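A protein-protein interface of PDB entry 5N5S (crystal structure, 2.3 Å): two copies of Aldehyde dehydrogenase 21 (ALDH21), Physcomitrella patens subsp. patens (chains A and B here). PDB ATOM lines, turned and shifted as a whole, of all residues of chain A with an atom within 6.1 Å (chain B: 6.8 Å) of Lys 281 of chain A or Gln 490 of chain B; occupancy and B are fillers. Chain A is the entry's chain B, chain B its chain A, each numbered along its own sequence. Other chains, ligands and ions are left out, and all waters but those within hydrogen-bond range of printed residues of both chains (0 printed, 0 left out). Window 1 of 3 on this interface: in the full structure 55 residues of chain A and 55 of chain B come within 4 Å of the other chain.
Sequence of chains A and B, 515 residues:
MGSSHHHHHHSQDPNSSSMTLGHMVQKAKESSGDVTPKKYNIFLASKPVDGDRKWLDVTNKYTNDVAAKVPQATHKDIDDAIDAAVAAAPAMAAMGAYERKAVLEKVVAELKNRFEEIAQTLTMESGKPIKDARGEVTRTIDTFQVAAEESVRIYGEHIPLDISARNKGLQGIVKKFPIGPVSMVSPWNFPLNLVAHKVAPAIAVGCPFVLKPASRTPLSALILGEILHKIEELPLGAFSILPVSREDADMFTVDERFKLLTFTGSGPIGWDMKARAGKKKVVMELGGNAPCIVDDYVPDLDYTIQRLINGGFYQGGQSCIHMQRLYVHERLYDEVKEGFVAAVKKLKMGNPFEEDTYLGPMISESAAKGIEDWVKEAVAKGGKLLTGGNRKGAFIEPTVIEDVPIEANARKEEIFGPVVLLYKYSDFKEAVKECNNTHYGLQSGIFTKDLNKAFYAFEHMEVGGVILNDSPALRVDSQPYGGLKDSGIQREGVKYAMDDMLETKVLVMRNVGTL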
ATOM      1  N   ILE A 179     -23.241 -15.295  31.108  1.00  0.00           N
ATOM      2  CA  ILE A 179     -23.085 -14.633  29.809  1.00  0.00           C
ATOM      3  C   ILE A 179     -23.158 -13.097  29.942  1.00  0.00           C
ATOM      4  O   ILE A 179     -22.422 -12.386  29.248  1.00  0.00           O
ATOM      5  CB  ILE A 179     -24.088 -15.216  28.747  1.00  0.00           C
ATOM      6  CG1 ILE A 179     -23.631 -14.885  27.299  1.00  0.00           C
ATOM      7  CG2 ILE A 179     -25.567 -14.810  29.015  1.00  0.00           C
ATOM      8  CD1 ILE A 179     -24.399 -15.636  26.169  1.00  0.00           C
ATOM      9  N   PHE A 258     -27.193  -6.258  25.721  1.00  0.00           N
ATOM     10  CA  PHE A 258     -27.672  -7.593  26.044  1.00  0.00           C
ATOM     11  C   PHE A 258     -26.721  -8.584  25.363  1.00  0.00           C
ATOM     12  O   PHE A 258     -26.379  -8.404  24.184  1.00  0.00           O
ATOM     13  CB  PHE A 258     -29.092  -7.822  25.520  1.00  0.00           C
ATOM     14  CG  PHE A 258     -30.229  -7.053  26.152  1.00  0.00           C
ATOM     15  CD1 PHE A 258     -30.578  -7.266  27.482  1.00  0.00           C
ATOM     16  CD2 PHE A 258     -31.044  -6.228  25.381  1.00  0.00           C
ATOM     17  CE1 PHE A 258     -31.689  -6.624  28.043  1.00  0.00           C
ATOM     18  CE2 PHE A 258     -32.162  -5.606  25.938  1.00  0.00           C
ATOM     19  CZ  PHE A 258     -32.478  -5.811  27.265  1.00  0.00           C
ATOM     20  N   LYS A 259     -26.294  -9.624  26.104  1.00  0.00           N
ATOM     21  CA  LYS A 259     -25.397 -10.654  25.577  1.00  0.00           C
ATOM     22  C   LYS A 259     -26.181 -11.857  25.041  1.00  0.00           C
ATOM     23  O   LYS A 259     -25.641 -12.669  24.286  1.00  0.00           O
ATOM     24  CB  LYS A 259     -24.340 -11.058  26.622  1.00  0.00           C
ATOM     25  CG  LYS A 259     -23.380  -9.917  27.033  1.00  0.00           C
ATOM     26  CD  LYS A 259     -22.457  -9.403  25.894  1.00  0.00           C
ATOM     27  CE  LYS A 259     -21.212 -10.223  25.533  1.00  0.00           C
ATOM     28  NZ  LYS A 259     -20.202 -10.260  26.626  1.00  0.00           N
ATOM     29  N   LEU A 260     -27.467 -11.939  25.405  1.00  0.00           N
ATOM     30  CA  LEU A 260     -28.372 -12.986  24.965  1.00  0.00           C
ATOM     31  C   LEU A 260     -29.799 -12.466  24.841  1.00  0.00           C
ATOM     32  O   LEU A 260     -30.257 -11.684  25.678  1.00  0.00           O
ATOM     33  CB  LEU A 260     -28.317 -14.204  25.924  1.00  0.00           C
ATOM     34  CG  LEU A 260     -29.386 -15.314  25.749  1.00  0.00           C
ATOM     35  CD1 LEU A 260     -29.011 -16.289  24.642  1.00  0.00           C
ATOM     36  CD2 LEU A 260     -29.612 -16.057  27.033  1.00  0.00           C
ATOM     37  N   LEU A 261     -30.487 -12.916  23.794  1.00  0.00           N
ATOM     38  CA  LEU A 261     -31.896 -12.684  23.561  1.00  0.00           C
ATOM     39  C   LEU A 261     -32.577 -14.062  23.606  1.00  0.00           C
ATOM     40  O   LEU A 261     -32.214 -14.969  22.849  1.00  0.00           O
ATOM     41  CB  LEU A 261     -32.163 -11.982  22.202  1.00  0.00           C
ATOM     42  CG  LEU A 261     -33.615 -12.037  21.657  1.00  0.00           C
ATOM     43  CD1 LEU A 261     -34.590 -11.235  22.536  1.00  0.00           C
ATOM     44  CD2 LEU A 261     -33.675 -11.556  20.228  1.00  0.00           C
ATOM     45  N   THR A 262     -33.522 -14.227  24.524  1.00  0.00           N
ATOM     46  CA  THR A 262     -34.295 -15.464  24.621  1.00  0.00           C
ATOM     47  C   THR A 262     -35.751 -15.108  24.335  1.00  0.00           C
ATOM     48  O   THR A 262     -36.367 -14.320  25.057  1.00  0.00           O
ATOM     49  CB  THR A 262     -34.001 -16.282  25.907  1.00  0.00           C
ATOM     50  OG1 THR A 262     -34.841 -17.435  25.934  1.00  0.00           O
ATOM     51  CG2 THR A 262     -34.129 -15.481  27.200  1.00  0.00           C
ATOM     52  N   ALA A 277     -30.941  -9.098  15.657  1.00  0.00           N
ATOM     53  CA  ALA A 277     -30.312  -9.244  16.975  1.00  0.00           C
ATOM     54  C   ALA A 277     -28.868  -8.718  17.119  1.00  0.00           C
ATOM     55  O   ALA A 277     -28.441  -8.412  18.237  1.00  0.00           O
ATOM     56  CB  ALA A 277     -30.365 -10.696  17.417  1.00  0.00           C
ATOM     57  N   LYS A 279     -24.815  -8.983  17.353  1.00  0.00           N
ATOM     58  CA  LYS A 279     -23.766  -9.860  17.885  1.00  0.00           C
ATOM     59  C   LYS A 279     -24.213 -10.904  18.916  1.00  0.00           C
ATOM     60  O   LYS A 279     -23.633 -11.992  18.958  1.00  0.00           O
ATOM     61  CB  LYS A 279     -22.630  -9.004  18.484  1.00  0.00           C
ATOM     62  CG  LYS A 279     -21.879  -8.202  17.434  1.00  0.00           C
ATOM     63  CD  LYS A 279     -20.682  -7.439  17.984  1.00  0.00           C
ATOM     64  CE  LYS A 279     -20.174  -6.445  16.962  1.00  0.00           C
ATOM     65  NZ  LYS A 279     -19.846  -5.122  17.570  1.00  0.00           N
ATOM     66  N   LYS A 280     -25.222 -10.573  19.749  1.00  0.00           N
ATOM     67  CA  LYS A 280     -25.733 -11.415  20.843  1.00  0.00           C
ATOM     68  C   LYS A 280     -26.148 -12.851  20.465  1.00  0.00           C
ATOM     69  O   LYS A 280     -26.542 -13.124  19.326  1.00  0.00           O
ATOM     70  CB  LYS A 280     -26.900 -10.725  21.576  1.00  0.00           C
ATOM     71  CG  LYS A 280     -28.143 -10.497  20.720  1.00  0.00           C
ATOM     72  CD  LYS A 280     -29.325  -9.883  21.482  1.00  0.00           C
ATOM     73  CE  LYS A 280     -29.184  -8.455  21.963  1.00  0.00           C
ATOM     74  NZ  LYS A 280     -28.655  -7.528  20.925  1.00  0.00           N
ATOM     75  N   LYS A 281     -26.082 -13.766  21.459  1.00  0.00           N
ATOM     76  CA  LYS A 281     -26.547 -15.126  21.272  1.00  0.00           C
ATOM     77  C   LYS A 281     -28.084 -15.086  21.266  1.00  0.00           C
ATOM     78  O   LYS A 281     -28.692 -14.164  21.816  1.00  0.00           O
ATOM     79  CB  LYS A 281     -25.988 -16.096  22.334  1.00  0.00           C
ATOM     80  CG  LYS A 281     -24.511 -16.429  22.134  1.00  0.00           C
ATOM     81  CD  LYS A 281     -24.036 -17.603  23.001  1.00  0.00           C
ATOM     82  CE  LYS A 281     -22.523 -17.681  23.049  1.00  0.00           C
ATOM     83  NZ  LYS A 281     -22.041 -18.939  23.672  1.00  0.00           N
ATOM     84  N   VAL A 282     -28.699 -16.061  20.599  1.00  0.00           N
ATOM     85  CA  VAL A 282     -30.147 -16.142  20.444  1.00  0.00           C
ATOM     86  C   VAL A 282     -30.671 -17.550  20.795  1.00  0.00           C
ATOM     87  O   VAL A 282     -30.025 -18.558  20.489  1.00  0.00           O
ATOM     88  CB  VAL A 282     -30.513 -15.659  19.004  1.00  0.00           C
ATOM     89  CG1 VAL A 282     -31.707 -16.389  18.411  1.00  0.00           C
ATOM     90  CG2 VAL A 282     -30.716 -14.150  18.962  1.00  0.00           C
ATOM     91  N   VAL A 283     -31.822 -17.580  21.493  1.00  0.00           N
ATOM     92  CA  VAL A 283     -32.600 -18.760  21.869  1.00  0.00           C
ATOM     93  C   VAL A 283     -33.987 -18.484  21.293  1.00  0.00           C
ATOM     94  O   VAL A 283     -34.557 -17.416  21.567  1.00  0.00           O
ATOM     95  CB  VAL A 283     -32.645 -18.993  23.410  1.00  0.00           C
ATOM     96  CG1 VAL A 283     -33.562 -20.172  23.773  1.00  0.00           C
ATOM     97  CG2 VAL A 283     -31.248 -19.216  23.975  1.00  0.00           C
ATOM     98  N   GLN A 490     -31.953 -23.981  19.819  1.00  0.00           N
ATOM     99  CA  GLN A 490     -31.569 -24.132  21.237  1.00  0.00           C
ATOM    100  C   GLN A 490     -32.643 -24.859  22.043  1.00  0.00           C
ATOM    101  O   GLN A 490     -33.687 -25.238  21.502  1.00  0.00           O
ATOM    102  CB  GLN A 490     -31.133 -22.797  21.907  1.00  0.00           C
ATOM    103  CG  GLN A 490     -30.066 -22.001  21.160  1.00  0.00           C
ATOM    104  CD  GLN A 490     -28.820 -22.782  20.856  1.00  0.00           C
ATOM    105  OE1 GLN A 490     -28.015 -23.108  21.731  1.00  0.00           O
ATOM    106  NE2 GLN A 490     -28.585 -22.998  19.587  1.00  0.00           N
ATOM    107  N   ASP A 500     -27.144 -22.008  27.854  1.00  0.00           N
ATOM    108  CA  ASP A 500     -27.142 -20.888  26.906  1.00  0.00           C
ATOM    109  C   ASP A 500     -26.810 -19.560  27.615  1.00  0.00           C
ATOM    110  O   ASP A 500     -26.338 -18.622  26.970  1.00  0.00           O
ATOM    111  CB  ASP A 500     -28.489 -20.806  26.156  1.00  0.00           C
ATOM    112  CG  ASP A 500     -28.878 -22.049  25.353  1.00  0.00           C
ATOM    113  OD1 ASP A 500     -27.999 -22.603  24.648  1.00  0.00           O
ATOM    114  OD2 ASP A 500     -30.081 -22.438  25.391  1.00  0.00           O
ATOM    115  N   LEU A 502     -24.582 -19.431  30.083  1.00  0.00           N
ATOM    116  CA  LEU A 502     -23.230 -19.631  30.582  1.00  0.00           C
ATOM    117  C   LEU A 502     -22.231 -19.647  29.441  1.00  0.00           C
ATOM    118  O   LEU A 502     -22.494 -20.230  28.397  1.00  0.00           O
ATOM    119  CB  LEU A 502     -23.132 -20.956  31.372  1.00  0.00           C
ATOM    120  CG  LEU A 502     -23.777 -20.985  32.769  1.00  0.00           C
ATOM    121  CD1 LEU A 502     -24.057 -22.396  33.199  1.00  0.00           C
ATOM    122  CD2 LEU A 502     -22.923 -20.252  33.818  1.00  0.00           C
ATOM    123  N   GLU A 503     -21.083 -19.001  29.649  1.00  0.00           N
ATOM    124  CA  GLU A 503     -19.943 -18.963  28.730  1.00  0.00           C
ATOM    125  C   GLU A 503     -18.832 -19.841  29.316  1.00  0.00           C
ATOM    126  O   GLU A 503     -18.599 -19.811  30.521  1.00  0.00           O
ATOM    127  CB  GLU A 503     -19.433 -17.526  28.513  1.00  0.00           C
ATOM    128  CG  GLU A 503     -20.326 -16.684  27.610  1.00  0.00           C
ATOM    129  CD  GLU A 503     -20.075 -16.724  26.113  1.00  0.00           C
ATOM    130  OE1 GLU A 503     -19.733 -17.808  25.583  1.00  0.00           O
ATOM    131  OE2 GLU A 503     -20.246 -15.662  25.464  1.00  0.00           O
ATOM    132  N   LEU B 260     -26.051 -24.981   9.622  1.00  0.00           N
ATOM    133  CA  LEU B 260     -25.007 -24.349  10.408  1.00  0.00           C
ATOM    134  C   LEU B 260     -23.975 -23.669   9.510  1.00  0.00           C
ATOM    135  O   LEU B 260     -23.593 -24.208   8.462  1.00  0.00           O
ATOM    136  CB  LEU B 260     -24.321 -25.365  11.360  1.00  0.00           C
ATOM    137  CG  LEU B 260     -23.029 -24.904  12.091  1.00  0.00           C
ATOM    138  CD1 LEU B 260     -23.344 -24.089  13.343  1.00  0.00           C
ATOM    139  CD2 LEU B 260     -22.155 -26.075  12.449  1.00  0.00           C
ATOM    140  N   LYS B 274     -23.097 -13.204  10.317  1.00  0.00           N
ATOM    141  CA  LYS B 274     -24.055 -13.653  11.335  1.00  0.00           C
ATOM    142  C   LYS B 274     -25.403 -12.935  11.114  1.00  0.00           C
ATOM    143  O   LYS B 274     -26.463 -13.567  11.211  1.00  0.00           O
ATOM    144  CB  LYS B 274     -23.510 -13.374  12.750  1.00  0.00           C
ATOM    145  CG  LYS B 274     -24.433 -13.825  13.882  1.00  0.00           C
ATOM    146  CD  LYS B 274     -23.906 -13.384  15.234  1.00  0.00           C
ATOM    147  CE  LYS B 274     -24.692 -13.955  16.391  1.00  0.00           C
ATOM    148  NZ  LYS B 274     -25.945 -13.179  16.639  1.00  0.00           N
ATOM    149  N   VAL B 282     -24.970 -20.445  14.086  1.00  0.00           N
ATOM    150  CA  VAL B 282     -23.725 -19.777  13.730  1.00  0.00           C
ATOM    151  C   VAL B 282     -22.641 -20.027  14.780  1.00  0.00           C
ATOM    152  O   VAL B 282     -22.930 -20.054  15.977  1.00  0.00           O
ATOM    153  CB  VAL B 282     -24.034 -18.262  13.454  1.00  0.00           C
ATOM    154  CG1 VAL B 282     -22.911 -17.333  13.875  1.00  0.00           C
ATOM    155  CG2 VAL B 282     -24.426 -18.022  11.999  1.00  0.00           C
ATOM    156  N   VAL B 283     -21.402 -20.256  14.307  1.00  0.00           N
ATOM    157  CA  VAL B 283     -20.169 -20.420  15.090  1.00  0.00           C
ATOM    158  C   VAL B 283     -19.232 -19.366  14.523  1.00  0.00           C
ATOM    159  O   VAL B 283     -19.029 -19.334  13.303  1.00  0.00           O
ATOM    160  CB  VAL B 283     -19.562 -21.856  14.982  1.00  0.00           C
ATOM    161  CG1 VAL B 283     -18.220 -21.953  15.719  1.00  0.00           C
ATOM    162  CG2 VAL B 283     -20.531 -22.909  15.498  1.00  0.00           C
ATOM    163  N   MET B 284     -18.712 -18.472  15.391  1.00  0.00           N
ATOM    164  CA  MET B 284     -17.825 -17.362  15.006  1.00  0.00           C
ATOM    165  C   MET B 284     -16.480 -17.389  15.728  1.00  0.00           C
ATOM    166  O   MET B 284     -16.411 -17.141  16.932  1.00  0.00           O
ATOM    167  CB  MET B 284     -18.516 -16.000  15.218  1.00  0.00           C
ATOM    168  CG  MET B 284     -19.628 -15.718  14.223  1.00  0.00           C
ATOM    169  SD  MET B 284     -19.010 -15.396  12.571  1.00  0.00           S
ATOM    170  CE  MET B 284     -20.327 -16.035  11.589  1.00  0.00           C
ATOM    171  N   GLU B 285     -15.409 -17.678  14.982  1.00  0.00           N
ATOM    172  CA  GLU B 285     -14.038 -17.681  15.489  1.00  0.00           C
ATOM    173  C   GLU B 285     -13.368 -16.459  14.860  1.00  0.00           C
ATOM    174  O   GLU B 285     -12.967 -16.499  13.697  1.00  0.00           O
ATOM    175  CB  GLU B 285     -13.328 -19.005  15.120  1.00  0.00           C
ATOM    176  CG  GLU B 285     -13.746 -20.203  15.959  1.00  0.00           C
ATOM    177  CD  GLU B 285     -13.365 -20.188  17.431  1.00  0.00           C
ATOM    178  OE1 GLU B 285     -14.068 -20.856  18.219  1.00  0.00           O
ATOM    179  OE2 GLU B 285     -12.380 -19.512  17.802  1.00  0.00           O
ATOM    180  N   TYR B 481     -11.969 -23.648  22.749  1.00  0.00           N
ATOM    181  CA  TYR B 481     -11.333 -22.453  22.188  1.00  0.00           C
ATOM    182  C   TYR B 481     -12.339 -21.553  21.487  1.00  0.00           C
ATOM    183  O   TYR B 481     -13.068 -21.998  20.614  1.00  0.00           O
ATOM    184  CB  TYR B 481     -10.214 -22.882  21.231  1.00  0.00           C
ATOM    185  CG  TYR B 481      -9.457 -21.748  20.583  1.00  0.00           C
ATOM    186  CD1 TYR B 481      -8.344 -21.183  21.200  1.00  0.00           C
ATOM    187  CD2 TYR B 481      -9.839 -21.249  19.340  1.00  0.00           C
ATOM    188  CE1 TYR B 481      -7.613 -20.167  20.586  1.00  0.00           C
ATOM    189  CE2 TYR B 481      -9.125 -20.219  18.723  1.00  0.00           C
ATOM    190  CZ  TYR B 481      -8.009 -19.690  19.347  1.00  0.00           C
ATOM    191  OH  TYR B 481      -7.300 -18.690  18.735  1.00  0.00           O
ATOM    192  N   GLY B 482     -12.327 -20.280  21.848  1.00  0.00           N
ATOM    193  CA  GLY B 482     -13.236 -19.297  21.286  1.00  0.00           C
ATOM    194  C   GLY B 482     -13.184 -18.017  22.062  1.00  0.00           C
ATOM    195  O   GLY B 482     -12.437 -17.914  23.035  1.00  0.00           O
ATOM    196  N   GLY B 483     -13.956 -17.033  21.626  1.00  0.00           N
ATOM    197  CA  GLY B 483     -13.898 -15.734  22.269  1.00  0.00           C
ATOM    198  C   GLY B 483     -15.151 -15.204  22.908  1.00  0.00           C
ATOM    199  O   GLY B 483     -16.239 -15.757  22.751  1.00  0.00           O
ATOM    200  N   GLY B 488     -15.945 -13.387  19.030  1.00  0.00           N
ATOM    201  CA  GLY B 488     -16.856 -14.409  18.539  1.00  0.00           C
ATOM    202  C   GLY B 488     -17.908 -14.897  19.498  1.00  0.00           C
ATOM    203  O   GLY B 488     -18.224 -14.238  20.490  1.00  0.00           O
ATOM    204  N   ILE B 489     -18.483 -16.054  19.145  1.00  0.00           N
ATOM    205  CA  ILE B 489     -19.502 -16.851  19.848  1.00  0.00           C
ATOM    206  C   ILE B 489     -19.227 -18.328  19.564  1.00  0.00           C
ATOM    207  O   ILE B 489     -18.785 -18.667  18.465  1.00  0.00           O
ATOM    208  CB  ILE B 489     -20.983 -16.485  19.521  1.00  0.00           C
ATOM    209  CG1 ILE B 489     -21.280 -16.516  18.006  1.00  0.00           C
ATOM    210  CG2 ILE B 489     -21.401 -15.150  20.158  1.00  0.00           C
ATOM    211  CD1 ILE B 489     -22.715 -16.849  17.684  1.00  0.00           C
ATOM    212  N   GLN B 490     -19.495 -19.194  20.553  1.00  0.00           N
ATOM    213  CA  GLN B 490     -19.327 -20.659  20.519  1.00  0.00           C
ATOM    214  C   GLN B 490     -17.862 -21.074  20.694  1.00  0.00           C
ATOM    215  O   GLN B 490     -16.978 -20.220  20.811  1.00  0.00           O
ATOM    216  CB  GLN B 490     -19.985 -21.331  19.279  1.00  0.00           C
ATOM    217  CG  GLN B 490     -21.461 -20.987  19.036  1.00  0.00           C
ATOM    218  CD  GLN B 490     -22.337 -21.222  20.242  1.00  0.00           C
ATOM    219  OE1 GLN B 490     -22.866 -20.282  20.841  1.00  0.00           O
ATOM    220  NE2 GLN B 490     -22.482 -22.477  20.649  1.00  0.00           N
ATOM    221  N   ARG B 491     -17.613 -22.382  20.755  1.00  0.00           N
ATOM    222  CA  ARG B 491     -16.288 -22.930  20.977  1.00  0.00           C
ATOM    223  C   ARG B 491     -15.906 -24.024  20.002  1.00  0.00           C
ATOM    224  O   ARG B 491     -16.692 -24.950  19.735  1.00  0.00           O
ATOM    225  CB  ARG B 491     -16.155 -23.505  22.421  1.00  0.00           C
ATOM    226  CG  ARG B 491     -16.311 -22.497  23.575  1.00  0.00           C
ATOM    227  CD  ARG B 491     -15.200 -21.449  23.621  1.00  0.00           C
ATOM    228  NE  ARG B 491     -15.426 -20.463  24.673  1.00  0.00           N
ATOM    229  CZ  ARG B 491     -16.096 -19.329  24.509  1.00  0.00           C
ATOM    230  NH1 ARG B 491     -16.597 -19.007  23.320  1.00  0.00           N
ATOM    231  NH2 ARG B 491     -16.262 -18.498  25.529  1.00  0.00           N
ATOM    232  N   GLU B 492     -14.669 -23.926  19.504  1.00  0.00           N
ATOM    233  CA  GLU B 492     -13.999 -24.946  18.709  1.00  0.00           C
ATOM    234  C   GLU B 492     -13.158 -25.770  19.701  1.00  0.00           C
ATOM    235  O   GLU B 492     -13.277 -25.566  20.907  1.00  0.00           O
ATOM    236  CB  GLU B 492     -13.227 -24.366  17.520  1.00  0.00           C
ATOM    237  CG  GLU B 492     -14.154 -24.105  16.344  1.00  0.00           C
ATOM    238  CD  GLU B 492     -13.493 -23.930  14.990  1.00  0.00           C
ATOM    239  OE1 GLU B 492     -12.246 -23.834  14.918  1.00  0.00           O
ATOM    240  OE2 GLU B 492     -14.237 -23.900  13.988  1.00  0.00           O
ATOM    241  N   TYR B 496     -16.085 -29.894  21.473  1.00  0.00           N
ATOM    242  CA  TYR B 496     -16.905 -28.681  21.609  1.00  0.00           C
ATOM    243  C   TYR B 496     -17.529 -28.282  20.262  1.00  0.00           C
ATOM    244  O   TYR B 496     -18.715 -27.926  20.221  1.00  0.00           O
ATOM    245  CB  TYR B 496     -16.088 -27.532  22.239  1.00  0.00           C
ATOM    246  CG  TYR B 496     -15.444 -27.912  23.555  1.00  0.00           C
ATOM    247  CD1 TYR B 496     -16.157 -27.832  24.750  1.00  0.00           C
ATOM    248  CD2 TYR B 496     -14.142 -28.409  23.602  1.00  0.00           C
ATOM    249  CE1 TYR B 496     -15.590 -28.234  25.959  1.00  0.00           C
ATOM    250  CE2 TYR B 496     -13.575 -28.841  24.802  1.00  0.00           C
ATOM    251  CZ  TYR B 496     -14.296 -28.727  25.984  1.00  0.00           C
ATOM    252  OH  TYR B 496     -13.752 -29.119  27.191  1.00  0.00           O
ATOM    253  N   ASP B 500     -21.937 -28.238  18.566  1.00  0.00           N
ATOM    254  CA  ASP B 500     -22.644 -27.269  17.720  1.00  0.00           C
ATOM    255  C   ASP B 500     -23.193 -27.937  16.443  1.00  0.00           C
ATOM    256  O   ASP B 500     -24.154 -27.441  15.842  1.00  0.00           O
ATOM    257  CB  ASP B 500     -21.724 -26.073  17.383  1.00  0.00           C
ATOM    258  CG  ASP B 500     -21.186 -25.291  18.586  1.00  0.00           C
ATOM    259  OD1 ASP B 500     -21.983 -25.010  19.518  1.00  0.00           O
ATOM    260  OD2 ASP B 500     -19.971 -24.921  18.571  1.00  0.00           O
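The backbone carbonyl oxygen (O) of Lys 259 of chain A is in hydrogen-bond range of the backbone NH (N) of Lys 281 of chain A (3.1 Å).
O of Lys 281 of chain A is in hydrogen-bond range of N of Leu 261 of chain A, at 2.9 Å.
O of Gly 483 of chain B lies within hydrogen-bond range of NH1 of Arg 491 of chain B (3.3 Å).
The backbone NH (N) of Met 284 of chain B sits at hydrogen-bond distance from the backbone carbonyl oxygen (O) of Ile 489 of chain B, at 3.1 Å.
O of Ala 277 of chain A sits at hydrogen-bond distance from NZ of Lys 280 of chain A, 2.8 Å away.
The side-chain amide nitrogen of Gln 490 of chain B lies within hydrogen-bond range of the side-chain carboxylate of Asp 500 of chain B, at 2.8 Å.
Lys 281 of chain A touches Ile 489 of chain B (CG to CG2, 3.9 Å).
5 positions are printed for both chains.
Of the 5 pairs that touch across the chains among the printed residues, none has its exchanged pair printed and touching as well.
Of the 16 printed residues of chain A, 4 touch a printed residue of chain B.
Among the printed residues, Asp or Glu carboxylates within 4 Å of a Lys or Arg side-chain nitrogen of the other chain: Glu 503 of chain A with Arg 491 of chain B.
OE1 of Glu 503 of chain A lies within salt-bridge range of NH2 of Arg 491 of chain B.
NZ of Lys 274 of chain B is in hydrogen-bond range of O of Lys 280 of chain A (2.8 Å).
O of Lys 279 of chain A lies close to NZ of Lys 274 of chain B, 3.5 Å away.
The side-chain amide oxygen (OE1) of Gln 490 of chain B sits at hydrogen-bond distance from the side-chain amino group (NZ) of Lys 281 of chain A (3.2 Å).
Of the printed residues of chain B, Lys 279 of chain A touches Lys 274 (3.4 Å).
Of the printed residues of chain B, Lys 280 of chain A touches Lys 274.
Val 282 of chain A touches none of the printed residues of chain B.
Of the printed residues of chain B, Glu 503 of chain A touches Arg 491 (3.5 Å).
Of the printed residues of chain A, Lys 274 of chain B touches Lys 279 (3.4 Å) and Lys 280 (2.8 Å).
Gln 490 of chain B touches just one residue of chain A: Lys 281.
Of the printed residues of chain A, Arg 491 of chain B touches Glu 503 (3.5 Å).
The nearest residue of chain A that does not touch Gln 490 of chain B is Glu 503 of chain A (5.2 Å).
The nearest printed residue of chain A that does not touch Lys 274 of chain B is Lys 281 of chain A (4.9 Å).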
